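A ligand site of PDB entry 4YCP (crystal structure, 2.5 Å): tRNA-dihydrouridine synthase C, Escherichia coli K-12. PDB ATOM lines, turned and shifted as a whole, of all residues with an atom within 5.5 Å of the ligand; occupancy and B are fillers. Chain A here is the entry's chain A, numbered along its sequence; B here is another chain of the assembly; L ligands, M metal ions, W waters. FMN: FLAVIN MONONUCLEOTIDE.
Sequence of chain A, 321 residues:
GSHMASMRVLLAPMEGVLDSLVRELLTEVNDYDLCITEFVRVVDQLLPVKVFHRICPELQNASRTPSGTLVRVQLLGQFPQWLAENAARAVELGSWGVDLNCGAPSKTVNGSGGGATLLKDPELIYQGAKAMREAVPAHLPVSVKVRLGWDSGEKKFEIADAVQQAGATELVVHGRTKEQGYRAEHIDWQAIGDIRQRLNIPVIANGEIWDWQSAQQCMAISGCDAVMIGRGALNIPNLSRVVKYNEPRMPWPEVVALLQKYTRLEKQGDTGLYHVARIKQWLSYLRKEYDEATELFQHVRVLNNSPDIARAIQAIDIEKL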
ATOM      1  N   ALA A  12       6.939   0.244   4.625  1.00  0.00           N
ATOM      2  CA  ALA A  12       6.818  -1.211   4.538  1.00  0.00           C
ATOM      3  C   ALA A  12       7.825  -1.837   3.577  1.00  0.00           C
ATOM      4  O   ALA A  12       8.283  -1.184   2.640  1.00  0.00           O
ATOM      5  CB  ALA A  12       5.405  -1.607   4.123  1.00  0.00           C
ATOM      6  N   PRO A  13       8.174  -3.116   3.809  1.00  0.00           N
ATOM      7  CA  PRO A  13       8.914  -3.846   2.769  1.00  0.00           C
ATOM      8  C   PRO A  13       7.996  -4.089   1.584  1.00  0.00           C
ATOM      9  O   PRO A  13       6.860  -4.522   1.771  1.00  0.00           O
ATOM     10  CB  PRO A  13       9.286  -5.151   3.465  1.00  0.00           C
ATOM     11  CG  PRO A  13       8.257  -5.330   4.525  1.00  0.00           C
ATOM     12  CD  PRO A  13       7.845  -3.962   4.966  1.00  0.00           C
ATOM     13  N   MET A  14       8.472  -3.784   0.375  1.00  0.00           N
ATOM     14  CA  MET A  14       7.698  -4.031  -0.857  1.00  0.00           C
ATOM     15  C   MET A  14       8.608  -4.524  -1.970  1.00  0.00           C
ATOM     16  O   MET A  14       9.270  -3.740  -2.641  1.00  0.00           O
ATOM     17  CB  MET A  14       6.933  -2.799  -1.302  1.00  0.00           C
ATOM     18  CG  MET A  14       5.743  -2.466  -0.409  1.00  0.00           C
ATOM     19  SD  MET A  14       4.807  -1.045  -0.999  1.00  0.00           S
ATOM     20  CE  MET A  14       3.794  -1.787  -2.276  1.00  0.00           C
ATOM     21  N   GLU A  15       8.618  -5.847  -2.136  1.00  0.00           N
ATOM     22  CA  GLU A  15       9.419  -6.526  -3.152  1.00  0.00           C
ATOM     23  C   GLU A  15       9.020  -6.066  -4.563  1.00  0.00           C
ATOM     24  O   GLU A  15       7.833  -6.061  -4.909  1.00  0.00           O
ATOM     25  CB  GLU A  15       9.273  -8.042  -2.991  1.00  0.00           C
ATOM     26  CG  GLU A  15      10.117  -8.874  -3.950  1.00  0.00           C
ATOM     27  CD  GLU A  15       9.487  -9.043  -5.316  1.00  0.00           C
ATOM     28  OE1 GLU A  15       8.237  -9.138  -5.408  1.00  0.00           O
ATOM     29  OE2 GLU A  15      10.251  -9.078  -6.303  1.00  0.00           O
ATOM     30  N   VAL A  17       9.243  -3.003  -5.664  1.00  0.00           N
ATOM     31  CA  VAL A  17       8.695  -1.644  -5.636  1.00  0.00           C
ATOM     32  C   VAL A  17       9.606  -0.715  -4.854  1.00  0.00           C
ATOM     33  O   VAL A  17      10.186   0.203  -5.421  1.00  0.00           O
ATOM     34  CB  VAL A  17       7.260  -1.605  -5.043  1.00  0.00           C
ATOM     35  CG1 VAL A  17       6.667  -0.197  -5.133  1.00  0.00           C
ATOM     36  CG2 VAL A  17       6.370  -2.620  -5.765  1.00  0.00           C
ATOM     37  N   THR A  37      13.709  -3.537   4.007  1.00  0.00           N
ATOM     38  CA  THR A  37      14.144  -3.863   2.650  1.00  0.00           C
ATOM     39  C   THR A  37      13.211  -4.881   2.018  1.00  0.00           C
ATOM     40  O   THR A  37      12.372  -5.481   2.685  1.00  0.00           O
ATOM     41  CB  THR A  37      15.556  -4.484   2.591  1.00  0.00           C
ATOM     42  OG1 THR A  37      15.541  -5.795   3.181  1.00  0.00           O
ATOM     43  CG2 THR A  37      16.601  -3.600   3.270  1.00  0.00           C
ATOM     44  N   GLU A  38      13.403  -5.071   0.718  1.00  0.00           N
ATOM     45  CA  GLU A  38      12.818  -6.212   0.008  1.00  0.00           C
ATOM     46  C   GLU A  38      13.445  -7.472   0.656  1.00  0.00           C
ATOM     47  O   GLU A  38      14.597  -7.410   1.097  1.00  0.00           O
ATOM     48  CB  GLU A  38      13.146  -6.144  -1.482  1.00  0.00           C
ATOM     49  CG  GLU A  38      12.659  -4.879  -2.177  1.00  0.00           C
ATOM     50  CD  GLU A  38      13.260  -4.692  -3.558  1.00  0.00           C
ATOM     51  OE1 GLU A  38      14.403  -4.184  -3.648  1.00  0.00           O
ATOM     52  OE2 GLU A  38      12.581  -5.058  -4.546  1.00  0.00           O
ATOM     53  N   PHE A  39      12.697  -8.560   0.741  1.00  0.00           N
ATOM     54  CA  PHE A  39      13.173  -9.753   1.454  1.00  0.00           C
ATOM     55  C   PHE A  39      14.445 -10.338   0.845  1.00  0.00           C
ATOM     56  O   PHE A  39      14.592 -10.369  -0.392  1.00  0.00           O
ATOM     57  CB  PHE A  39      12.090 -10.846   1.594  1.00  0.00           C
ATOM     58  CG  PHE A  39      11.656 -11.472   0.291  1.00  0.00           C
ATOM     59  CD1 PHE A  39      12.345 -12.546  -0.268  1.00  0.00           C
ATOM     60  CD2 PHE A  39      10.504 -11.029  -0.350  1.00  0.00           C
ATOM     61  CE1 PHE A  39      11.922 -13.127  -1.451  1.00  0.00           C
ATOM     62  CE2 PHE A  39      10.065 -11.606  -1.534  1.00  0.00           C
ATOM     63  CZ  PHE A  39      10.782 -12.656  -2.084  1.00  0.00           C
ATOM     64  N   GLN A  74      15.295  -7.504   5.780  1.00  0.00           N
ATOM     65  CA  GLN A  74      14.336  -8.565   6.076  1.00  0.00           C
ATOM     66  C   GLN A  74      14.811  -9.881   5.481  1.00  0.00           C
ATOM     67  O   GLN A  74      15.282  -9.903   4.345  1.00  0.00           O
ATOM     68  CB  GLN A  74      12.949  -8.233   5.536  1.00  0.00           C
ATOM     69  CG  GLN A  74      11.900  -9.275   5.896  1.00  0.00           C
ATOM     70  CD  GLN A  74      10.576  -9.044   5.215  1.00  0.00           C
ATOM     71  OE1 GLN A  74      10.444  -9.253   4.020  1.00  0.00           O
ATOM     72  NE2 GLN A  74       9.576  -8.634   5.990  1.00  0.00           N
ATOM     73  N   ASP A  99      14.640  -8.166  10.207  1.00  0.00           N
ATOM     74  CA  ASP A  99      13.205  -8.515  10.207  1.00  0.00           C
ATOM     75  C   ASP A  99      13.037  -9.950   9.691  1.00  0.00           C
ATOM     76  O   ASP A  99      13.774 -10.365   8.805  1.00  0.00           O
ATOM     77  CB  ASP A  99      12.415  -7.518   9.328  1.00  0.00           C
ATOM     78  CG  ASP A  99      10.894  -7.572   9.570  1.00  0.00           C
ATOM     79  OD1 ASP A  99      10.462  -7.453  10.742  1.00  0.00           O
ATOM     80  OD2 ASP A  99      10.131  -7.700   8.577  1.00  0.00           O
ATOM     81  N   ASN A 101      10.307 -12.394   7.739  1.00  0.00           N
ATOM     82  CA  ASN A 101       9.076 -12.478   6.967  1.00  0.00           C
ATOM     83  C   ASN A 101       8.292 -13.729   7.352  1.00  0.00           C
ATOM     84  O   ASN A 101       8.787 -14.855   7.200  1.00  0.00           O
ATOM     85  CB  ASN A 101       9.403 -12.510   5.466  1.00  0.00           C
ATOM     86  CG  ASN A 101       8.158 -12.431   4.596  1.00  0.00           C
ATOM     87  OD1 ASN A 101       7.206 -13.200   4.764  1.00  0.00           O
ATOM     88  ND2 ASN A 101       8.166 -11.520   3.627  1.00  0.00           N
ATOM     89  N   LYS A 145       7.410  -9.875  10.979  1.00  0.00           N
ATOM     90  CA  LYS A 145       6.246  -9.344  10.272  1.00  0.00           C
ATOM     91  C   LYS A 145       5.340 -10.508   9.922  1.00  0.00           C
ATOM     92  O   LYS A 145       5.755 -11.439   9.227  1.00  0.00           O
ATOM     93  CB  LYS A 145       6.678  -8.577   9.025  1.00  0.00           C
ATOM     94  CG  LYS A 145       5.542  -7.821   8.362  1.00  0.00           C
ATOM     95  CD  LYS A 145       6.072  -6.821   7.356  1.00  0.00           C
ATOM     96  CE  LYS A 145       4.954  -6.128   6.612  1.00  0.00           C
ATOM     97  NZ  LYS A 145       4.405  -6.957   5.512  1.00  0.00           N
ATOM     98  N   HIS A 174       0.245  -7.426   9.778  1.00  0.00           N
ATOM     99  CA  HIS A 174      -0.596  -7.139   8.618  1.00  0.00           C
ATOM    100  C   HIS A 174      -1.966  -7.771   8.901  1.00  0.00           C
ATOM    101  O   HIS A 174      -2.075  -9.000   8.979  1.00  0.00           O
ATOM    102  CB  HIS A 174       0.053  -7.725   7.362  1.00  0.00           C
ATOM    103  CG  HIS A 174      -0.722  -7.535   6.096  1.00  0.00           C
ATOM    104  ND1 HIS A 174      -0.402  -8.198   4.932  1.00  0.00           N
ATOM    105  CD2 HIS A 174      -1.810  -6.779   5.812  1.00  0.00           C
ATOM    106  CE1 HIS A 174      -1.252  -7.847   3.982  1.00  0.00           C
ATOM    107  NE2 HIS A 174      -2.115  -6.985   4.485  1.00  0.00           N
ATOM    108  N   ARG A 176      -4.631  -9.159   7.923  1.00  0.00           N
ATOM    109  CA  ARG A 176      -5.362 -10.078   7.061  1.00  0.00           C
ATOM    110  C   ARG A 176      -4.678 -11.438   7.085  1.00  0.00           C
ATOM    111  O   ARG A 176      -3.533 -11.547   7.495  1.00  0.00           O
ATOM    112  CB  ARG A 176      -5.406  -9.559   5.625  1.00  0.00           C
ATOM    113  CG  ARG A 176      -6.549  -8.597   5.339  1.00  0.00           C
ATOM    114  CD  ARG A 176      -6.413  -7.950   3.961  1.00  0.00           C
ATOM    115  NE  ARG A 176      -5.415  -6.875   3.965  1.00  0.00           N
ATOM    116  CZ  ARG A 176      -5.403  -5.834   3.127  1.00  0.00           C
ATOM    117  NH1 ARG A 176      -6.339  -5.674   2.191  1.00  0.00           N
ATOM    118  NH2 ARG A 176      -4.442  -4.913   3.225  1.00  0.00           N
ATOM    119  N   TYR A 182      -5.013  -8.903  -0.572  1.00  0.00           N
ATOM    120  CA  TYR A 182      -5.044  -7.439  -0.474  1.00  0.00           C
ATOM    121  C   TYR A 182      -6.458  -6.854  -0.627  1.00  0.00           C
ATOM    122  O   TYR A 182      -6.612  -5.669  -0.935  1.00  0.00           O
ATOM    123  CB  TYR A 182      -4.066  -6.842  -1.494  1.00  0.00           C
ATOM    124  CG  TYR A 182      -2.648  -7.217  -1.163  1.00  0.00           C
ATOM    125  CD1 TYR A 182      -2.082  -8.387  -1.663  1.00  0.00           C
ATOM    126  CD2 TYR A 182      -1.890  -6.428  -0.295  1.00  0.00           C
ATOM    127  CE1 TYR A 182      -0.786  -8.751  -1.334  1.00  0.00           C
ATOM    128  CE2 TYR A 182      -0.598  -6.783   0.033  1.00  0.00           C
ATOM    129  CZ  TYR A 182      -0.045  -7.938  -0.476  1.00  0.00           C
ATOM    130  OH  TYR A 182       1.243  -8.270  -0.112  1.00  0.00           O
ATOM    131  N   ASN A 206      -0.646  -2.641  10.555  1.00  0.00           N
ATOM    132  CA  ASN A 206      -0.379  -2.552   9.131  1.00  0.00           C
ATOM    133  C   ASN A 206      -1.583  -2.979   8.293  1.00  0.00           C
ATOM    134  O   ASN A 206      -2.234  -3.967   8.609  1.00  0.00           O
ATOM    135  CB  ASN A 206       0.829  -3.425   8.788  1.00  0.00           C
ATOM    136  CG  ASN A 206       1.048  -3.548   7.304  1.00  0.00           C
ATOM    137  OD1 ASN A 206       0.991  -4.639   6.757  1.00  0.00           O
ATOM    138  ND2 ASN A 206       1.259  -2.418   6.633  1.00  0.00           N
ATOM    139  N   GLY A 207      -1.845  -2.229   7.217  1.00  0.00           N
ATOM    140  CA  GLY A 207      -2.888  -2.549   6.245  1.00  0.00           C
ATOM    141  C   GLY A 207      -3.935  -1.457   6.111  1.00  0.00           C
ATOM    142  O   GLY A 207      -4.536  -1.029   7.113  1.00  0.00           O
ATOM    143  N   GLU A 208      -4.156  -1.017   4.863  1.00  0.00           N
ATOM    144  CA  GLU A 208      -5.248  -0.103   4.490  1.00  0.00           C
ATOM    145  C   GLU A 208      -5.163   1.292   5.143  1.00  0.00           C
ATOM    146  O   GLU A 208      -6.188   1.924   5.414  1.00  0.00           O
ATOM    147  CB  GLU A 208      -6.621  -0.760   4.745  1.00  0.00           C
ATOM    148  CG  GLU A 208      -6.851  -2.062   3.993  1.00  0.00           C
ATOM    149  CD  GLU A 208      -6.882  -1.904   2.483  1.00  0.00           C
ATOM    150  OE1 GLU A 208      -7.461  -0.921   1.981  1.00  0.00           O
ATOM    151  OE2 GLU A 208      -6.324  -2.772   1.782  1.00  0.00           O
ATOM    152  N   ILE A 209      -3.956   1.772   5.377  1.00  0.00           N
ATOM    153  CA  ILE A 209      -3.728   3.132   5.836  1.00  0.00           C
ATOM    154  C   ILE A 209      -3.381   3.949   4.596  1.00  0.00           C
ATOM    155  O   ILE A 209      -2.294   3.799   4.032  1.00  0.00           O
ATOM    156  CB  ILE A 209      -2.605   3.196   6.893  1.00  0.00           C
ATOM    157  CG1 ILE A 209      -2.973   2.359   8.118  1.00  0.00           C
ATOM    158  CG2 ILE A 209      -2.320   4.644   7.296  1.00  0.00           C
ATOM    159  CD1 ILE A 209      -1.813   2.035   9.025  1.00  0.00           C
ATOM    160  N   TRP A 210      -4.329   4.792   4.164  1.00  0.00           N
ATOM    161  CA  TRP A 210      -4.204   5.551   2.910  1.00  0.00           C
ATOM    162  C   TRP A 210      -4.074   7.059   3.088  1.00  0.00           C
ATOM    163  O   TRP A 210      -3.686   7.747   2.138  1.00  0.00           O
ATOM    164  CB  TRP A 210      -5.421   5.292   2.037  1.00  0.00           C
ATOM    165  CG  TRP A 210      -5.664   3.838   1.779  1.00  0.00           C
ATOM    166  CD1 TRP A 210      -6.635   3.062   2.328  1.00  0.00           C
ATOM    167  CD2 TRP A 210      -4.912   2.992   0.899  1.00  0.00           C
ATOM    168  NE1 TRP A 210      -6.539   1.780   1.847  1.00  0.00           N
ATOM    169  CE2 TRP A 210      -5.501   1.710   0.965  1.00  0.00           C
ATOM    170  CE3 TRP A 210      -3.816   3.203   0.055  1.00  0.00           C
ATOM    171  CZ2 TRP A 210      -5.012   0.622   0.223  1.00  0.00           C
ATOM    172  CZ3 TRP A 210      -3.327   2.115  -0.687  1.00  0.00           C
ATOM    173  CH2 TRP A 210      -3.932   0.849  -0.601  1.00  0.00           C
ATOM    174  N   MET A 228       2.688   0.871  10.078  1.00  0.00           N
ATOM    175  CA  MET A 228       3.496   0.646   8.880  1.00  0.00           C
ATOM    176  C   MET A 228       2.603   0.851   7.662  1.00  0.00           C
ATOM    177  O   MET A 228       1.505   0.311   7.621  1.00  0.00           O
ATOM    178  CB  MET A 228       4.089  -0.767   8.892  1.00  0.00           C
ATOM    179  CG  MET A 228       4.771  -1.198   7.598  1.00  0.00           C
ATOM    180  SD  MET A 228       5.577  -2.805   7.723  1.00  0.00           S
ATOM    181  CE  MET A 228       7.099  -2.377   8.563  1.00  0.00           C
ATOM    182  N   ILE A 229       3.095   1.605   6.682  1.00  0.00           N
ATOM    183  CA  ILE A 229       2.329   1.856   5.450  1.00  0.00           C
ATOM    184  C   ILE A 229       3.128   1.416   4.215  1.00  0.00           C
ATOM    185  O   ILE A 229       4.322   1.714   4.092  1.00  0.00           O
ATOM    186  CB  ILE A 229       1.862   3.331   5.339  1.00  0.00           C
ATOM    187  CG1 ILE A 229       3.034   4.279   5.054  1.00  0.00           C
ATOM    188  CG2 ILE A 229       1.124   3.735   6.609  1.00  0.00           C
ATOM    189  CD1 ILE A 229       2.729   5.748   5.288  1.00  0.00           C
ATOM    190  N   GLY A 230       2.451   0.673   3.330  1.00  0.00           N
ATOM    191  CA  GLY A 230       3.049   0.143   2.104  1.00  0.00           C
ATOM    192  C   GLY A 230       2.518   0.839   0.862  1.00  0.00           C
ATOM    193  O   GLY A 230       3.050   1.877   0.459  1.00  0.00           O
ATOM    194  N   ARG A 231       1.447   0.289   0.278  1.00  0.00           N
ATOM    195  CA  ARG A 231       0.943   0.763  -1.027  1.00  0.00           C
ATOM    196  C   ARG A 231       0.514   2.227  -1.043  1.00  0.00           C
ATOM    197  O   ARG A 231       0.668   2.892  -2.079  1.00  0.00           O
ATOM    198  CB  ARG A 231      -0.222  -0.107  -1.495  1.00  0.00           C
ATOM    199  CG  ARG A 231       0.158  -1.538  -1.831  1.00  0.00           C
ATOM    200  CD  ARG A 231      -1.076  -2.406  -1.921  1.00  0.00           C
ATOM    201  NE  ARG A 231      -1.802  -2.424  -0.646  1.00  0.00           N
ATOM    202  CZ  ARG A 231      -3.085  -2.717  -0.494  1.00  0.00           C
ATOM    203  NH1 ARG A 231      -3.859  -3.040  -1.532  1.00  0.00           N
ATOM    204  NH2 ARG A 231      -3.618  -2.674   0.722  1.00  0.00           N
ATOM    205  N   GLY A 232      -0.024   2.723   0.068  1.00  0.00           N
ATOM    206  CA  GLY A 232      -0.357   4.142   0.223  1.00  0.00           C
ATOM    207  C   GLY A 232       0.826   5.103   0.073  1.00  0.00           C
ATOM    208  O   GLY A 232       0.649   6.250  -0.348  1.00  0.00           O
ATOM    209  N   TYR A 285       0.093   3.040  -9.322  1.00  0.00           N
ATOM    210  CA  TYR A 285      -0.304   3.383  -7.949  1.00  0.00           C
ATOM    211  C   TYR A 285      -0.890   4.805  -7.876  1.00  0.00           C
ATOM    212  O   TYR A 285      -1.974   4.999  -7.320  1.00  0.00           O
ATOM    213  CB  TYR A 285       0.872   3.269  -6.969  1.00  0.00           C
ATOM    214  CG  TYR A 285       1.267   1.854  -6.609  1.00  0.00           C
ATOM    215  CD1 TYR A 285       0.481   1.093  -5.728  1.00  0.00           C
ATOM    216  CD2 TYR A 285       2.415   1.274  -7.121  1.00  0.00           C
ATOM    217  CE1 TYR A 285       0.848  -0.192  -5.374  1.00  0.00           C
ATOM    218  CE2 TYR A 285       2.787  -0.021  -6.781  1.00  0.00           C
ATOM    219  CZ  TYR A 285       1.995  -0.752  -5.908  1.00  0.00           C
ATOM    220  OH  TYR A 285       2.377  -2.031  -5.582  1.00  0.00           O
ATOM    221  P     U B  16       7.672 -14.574  -5.759  1.00  0.00           P
ATOM    222  OP1   U B  16       7.366 -15.921  -5.245  1.00  0.00           O
ATOM    223  OP2   U B  16       7.487 -14.273  -7.206  1.00  0.00           O
ATOM    224  O5'   U B  16       6.856 -13.537  -4.882  1.00  0.00           O
ATOM    225  C5'   U B  16       6.693 -12.163  -5.288  1.00  0.00           C
ATOM    226  C4'   U B  16       5.243 -11.775  -5.167  1.00  0.00           C
ATOM    227  O4'   U B  16       4.803 -11.956  -3.796  1.00  0.00           O
ATOM    228  C3'   U B  16       4.942 -10.328  -5.507  1.00  0.00           C
ATOM    229  O3'   U B  16       3.604 -10.233  -5.973  1.00  0.00           O
ATOM    230  C2'   U B  16       5.029  -9.647  -4.152  1.00  0.00           C
ATOM    231  O2'   U B  16       4.297  -8.447  -4.111  1.00  0.00           O
ATOM    232  C1'   U B  16       4.412 -10.715  -3.250  1.00  0.00           C
ATOM    233  N1    U B  16       4.869 -10.666  -1.857  1.00  0.00           N
ATOM    234  C2    U B  16       3.946 -10.330  -0.883  1.00  0.00           C
ATOM    235  O2    U B  16       2.777 -10.069  -1.136  1.00  0.00           O
ATOM    236  N3    U B  16       4.432 -10.331   0.400  1.00  0.00           N
ATOM    237  C4    U B  16       5.713 -10.620   0.803  1.00  0.00           C
ATOM    238  O4    U B  16       5.994 -10.585   2.007  1.00  0.00           O
ATOM    239  C5    U B  16       6.619 -10.957  -0.250  1.00  0.00           C
ATOM    240  C6    U B  16       6.170 -10.972  -1.516  1.00  0.00           C
ATOM    241  P     U B  17       3.319 -10.093  -7.529  1.00  0.00           P
ATOM    242  OP1   U B  17       3.636 -11.396  -8.178  1.00  0.00           O
ATOM    243  OP2   U B  17       3.977  -8.860  -7.994  1.00  0.00           O
ATOM    244  O5'   U B  17       1.736  -9.873  -7.555  1.00  0.00           O
ATOM    245  C5'   U B  17       0.848 -10.878  -7.043  1.00  0.00           C
ATOM    246  C4'   U B  17      -0.535 -10.315  -6.888  1.00  0.00           C
ATOM    247  O4'   U B  17      -0.579  -9.400  -5.768  1.00  0.00           O
ATOM    248  C3'   U B  17      -1.063  -9.469  -8.020  1.00  0.00           C
ATOM    249  O3'   U B  17      -1.453 -10.250  -9.146  1.00  0.00           O
ATOM    250  C2'   U B  17      -2.226  -8.754  -7.350  1.00  0.00           C
ATOM    251  O2'   U B  17      -3.397  -9.553  -7.318  1.00  0.00           O
ATOM    252  C1'   U B  17      -1.681  -8.522  -5.943  1.00  0.00           C
ATOM    253  N1    U B  17      -1.218  -7.137  -5.723  1.00  0.00           N
ATOM    254  C2    U B  17      -2.104  -6.248  -5.145  1.00  0.00           C
ATOM    255  O2    U B  17      -3.228  -6.557  -4.804  1.00  0.00           O
ATOM    256  N3    U B  17      -1.627  -4.970  -4.985  1.00  0.00           N
ATOM    257  C4    U B  17      -0.377  -4.495  -5.336  1.00  0.00           C
ATOM    258  O4    U B  17      -0.089  -3.320  -5.116  1.00  0.00           O
ATOM    259  C5    U B  17       0.482  -5.474  -5.935  1.00  0.00           C
ATOM    260  C6    U B  17       0.041  -6.726  -6.107  1.00  0.00           C
HETATM  261  N1  FMN L   1       5.785  -7.709   2.986  1.00  0.00           N
HETATM  262  C2  FMN L   1       6.998  -8.226   3.406  1.00  0.00           C
HETATM  263  O2  FMN L   1       7.185  -8.565   4.571  1.00  0.00           O
HETATM  264  N3  FMN L   1       8.030  -8.366   2.505  1.00  0.00           N
HETATM  265  C4  FMN L   1       7.994  -8.046   1.160  1.00  0.00           C
HETATM  266  O4  FMN L   1       8.995  -8.177   0.468  1.00  0.00           O
HETATM  267  C4A FMN L   1       6.692  -7.517   0.712  1.00  0.00           C
HETATM  268  N5  FMN L   1       6.566  -7.200  -0.547  1.00  0.00           N
HETATM  269  C5A FMN L   1       5.351  -6.662  -0.961  1.00  0.00           C
HETATM  270  C6  FMN L   1       5.226  -6.250  -2.287  1.00  0.00           C
HETATM  271  C7  FMN L   1       4.045  -5.678  -2.755  1.00  0.00           C
HETATM  272  C7M FMN L   1       3.960  -5.255  -4.199  1.00  0.00           C
HETATM  273  C8  FMN L   1       2.962  -5.508  -1.879  1.00  0.00           C
HETATM  274  C8M FMN L   1       1.640  -4.967  -2.357  1.00  0.00           C
HETATM  275  C9  FMN L   1       3.089  -5.908  -0.547  1.00  0.00           C
HETATM  276  C9A FMN L   1       4.276  -6.476  -0.071  1.00  0.00           C
HETATM  277  N10 FMN L   1       4.453  -6.852   1.293  1.00  0.00           N
HETATM  278  C10 FMN L   1       5.647  -7.377   1.705  1.00  0.00           C
HETATM  279  C1' FMN L   1       3.383  -6.625   2.282  1.00  0.00           C
HETATM  280  C2' FMN L   1       3.450  -5.191   2.798  1.00  0.00           C
HETATM  281  O2' FMN L   1       4.618  -5.002   3.591  1.00  0.00           O
HETATM  282  C3' FMN L   1       2.212  -4.829   3.636  1.00  0.00           C
HETATM  283  O3' FMN L   1       2.125  -5.735   4.720  1.00  0.00           O
HETATM  284  C4' FMN L   1       0.896  -4.830   2.869  1.00  0.00           C
HETATM  285  O4' FMN L   1       1.043  -4.170   1.613  1.00  0.00           O
HETATM  286  C5' FMN L   1      -0.258  -4.215   3.642  1.00  0.00           C
HETATM  287  O5' FMN L   1       0.023  -2.823   3.870  1.00  0.00           O
HETATM  288  P   FMN L   1      -0.668  -1.683   2.987  1.00  0.00           P
HETATM  289  O1P FMN L   1      -2.145  -1.793   3.056  1.00  0.00           O
HETATM  290  O2P FMN L   1      -0.131  -0.365   3.540  1.00  0.00           O
HETATM  291  O3P FMN L   1      -0.146  -1.864   1.554  1.00  0.00           O
HETATM  292 MG    MG M   1       5.261  -7.327  -8.345  1.00  0.00          MG
HETATM  293  O   HOH W   1      -1.035   0.115   6.015  1.00  0.00           O
HETATM  294  O   HOH W   2      -0.698   1.989   2.559  1.00  0.00           O
HETATM  295  O   HOH W   3       5.497  -7.144  -6.184  1.00  0.00           O
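The side-chain amide nitrogen (ND2) of Asn 206 lies within hydrogen-bond range of the backbone carbonyl oxygen (O) of Met 228 (2.9 Å). The guanidinium group (NH2) of Arg 231 lies within salt-bridge range of the side-chain carboxylate (OE2) of Glu 208 (2.9 Å). The side-chain amide nitrogen (NE2) of Gln 74 is in hydrogen-bond range of the side-chain carboxylate (OD2) of Asp 99 (2.8 Å). O4 of U 17 of chain B is in hydrogen-bond range of the side-chain hydroxyl (OH) of Tyr 285, at 2.8 Å. The indole nitrogen of Trp 210 is in hydrogen-bond range of the side-chain carboxylate of Glu 208, 2.9 Å away. O4 of U 16 of chain B lies within hydrogen-bond range of ND2 of Asn 101 (2.9 Å). NE2 of His 174 sits at hydrogen-bond distance from NE of Arg 176. The backbone NH (N) of Gln 74 sits at hydrogen-bond distance from the side-chain hydroxyl (OG1) of Thr 37, at 3.1 Å.
Water W2 lies within hydrogen-bond range of O2P of the ligand, N of Gly 232, O of Ile 209 and N of Gly 230. Water W3 lies within hydrogen-bond range of O2' of U 16 of chain B and O of Glu 15.
Merely in contact with the ligand: Tyr 182, Phe 39, Gly 207, Met 14, His 174, Ala 12, U 17 of chain B, Ile 229, Tyr 285 and Val 17 of chain A. 21 residues have an atom within 4 Å of the ligand: Ala 12, Pro 13, Met 14, Glu 15, Val 17 of chain A, Phe 39, Gln 74, Asn 101, Lys 145, His 174, Arg 176, Tyr 182, Asn 206, Gly 207, Glu 208, Ile 229, Gly 230, Arg 231, Tyr 285, U 16 of chain B and U 17 of chain B.
The side-chain amide nitrogen (ND2) of Asn 101 lies within hydrogen-bond range of an oxygen (O2) of the ligand (3.3 Å). O1P of the ligand lies within hydrogen-bond range of N of Glu 208, at 2.8 Å. O4 of U 16 of chain B lies close to a nitrogen (N3) of the ligand, 3.1 Å away. An oxygen (O2P) of the ligand is in hydrogen-bond range of the backbone NH (N) of Gly 230 (2.8 Å). An oxygen (O1P) of the ligand is in salt-bridge range of the guanidinium group (NH2) of Arg 176, 3.9 Å away. The backbone NH (N) of Glu 15 is in hydrogen-bond range of a nitrogen (N5) of the ligand, at 2.9 Å. O of Pro 13 is in hydrogen-bond range of O2' of the ligand, 2.9 Å away. The side-chain amide oxygen (OD1) of Asn 206 sits at hydrogen-bond distance from an oxygen (O3') of the ligand (2.6 Å). The guanidinium group (NE) of Arg 231 is in salt-bridge range of an oxygen (O3P) of the ligand (2.8 Å). N of Arg 231 lies within hydrogen-bond range of O3P of the ligand, 3.0 Å away. NE2 of Gln 74 lies within hydrogen-bond range of O2 of the ligand. NZ of Lys 145 sits at hydrogen-bond distance from O3' of the ligand, at 2.7 Å.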
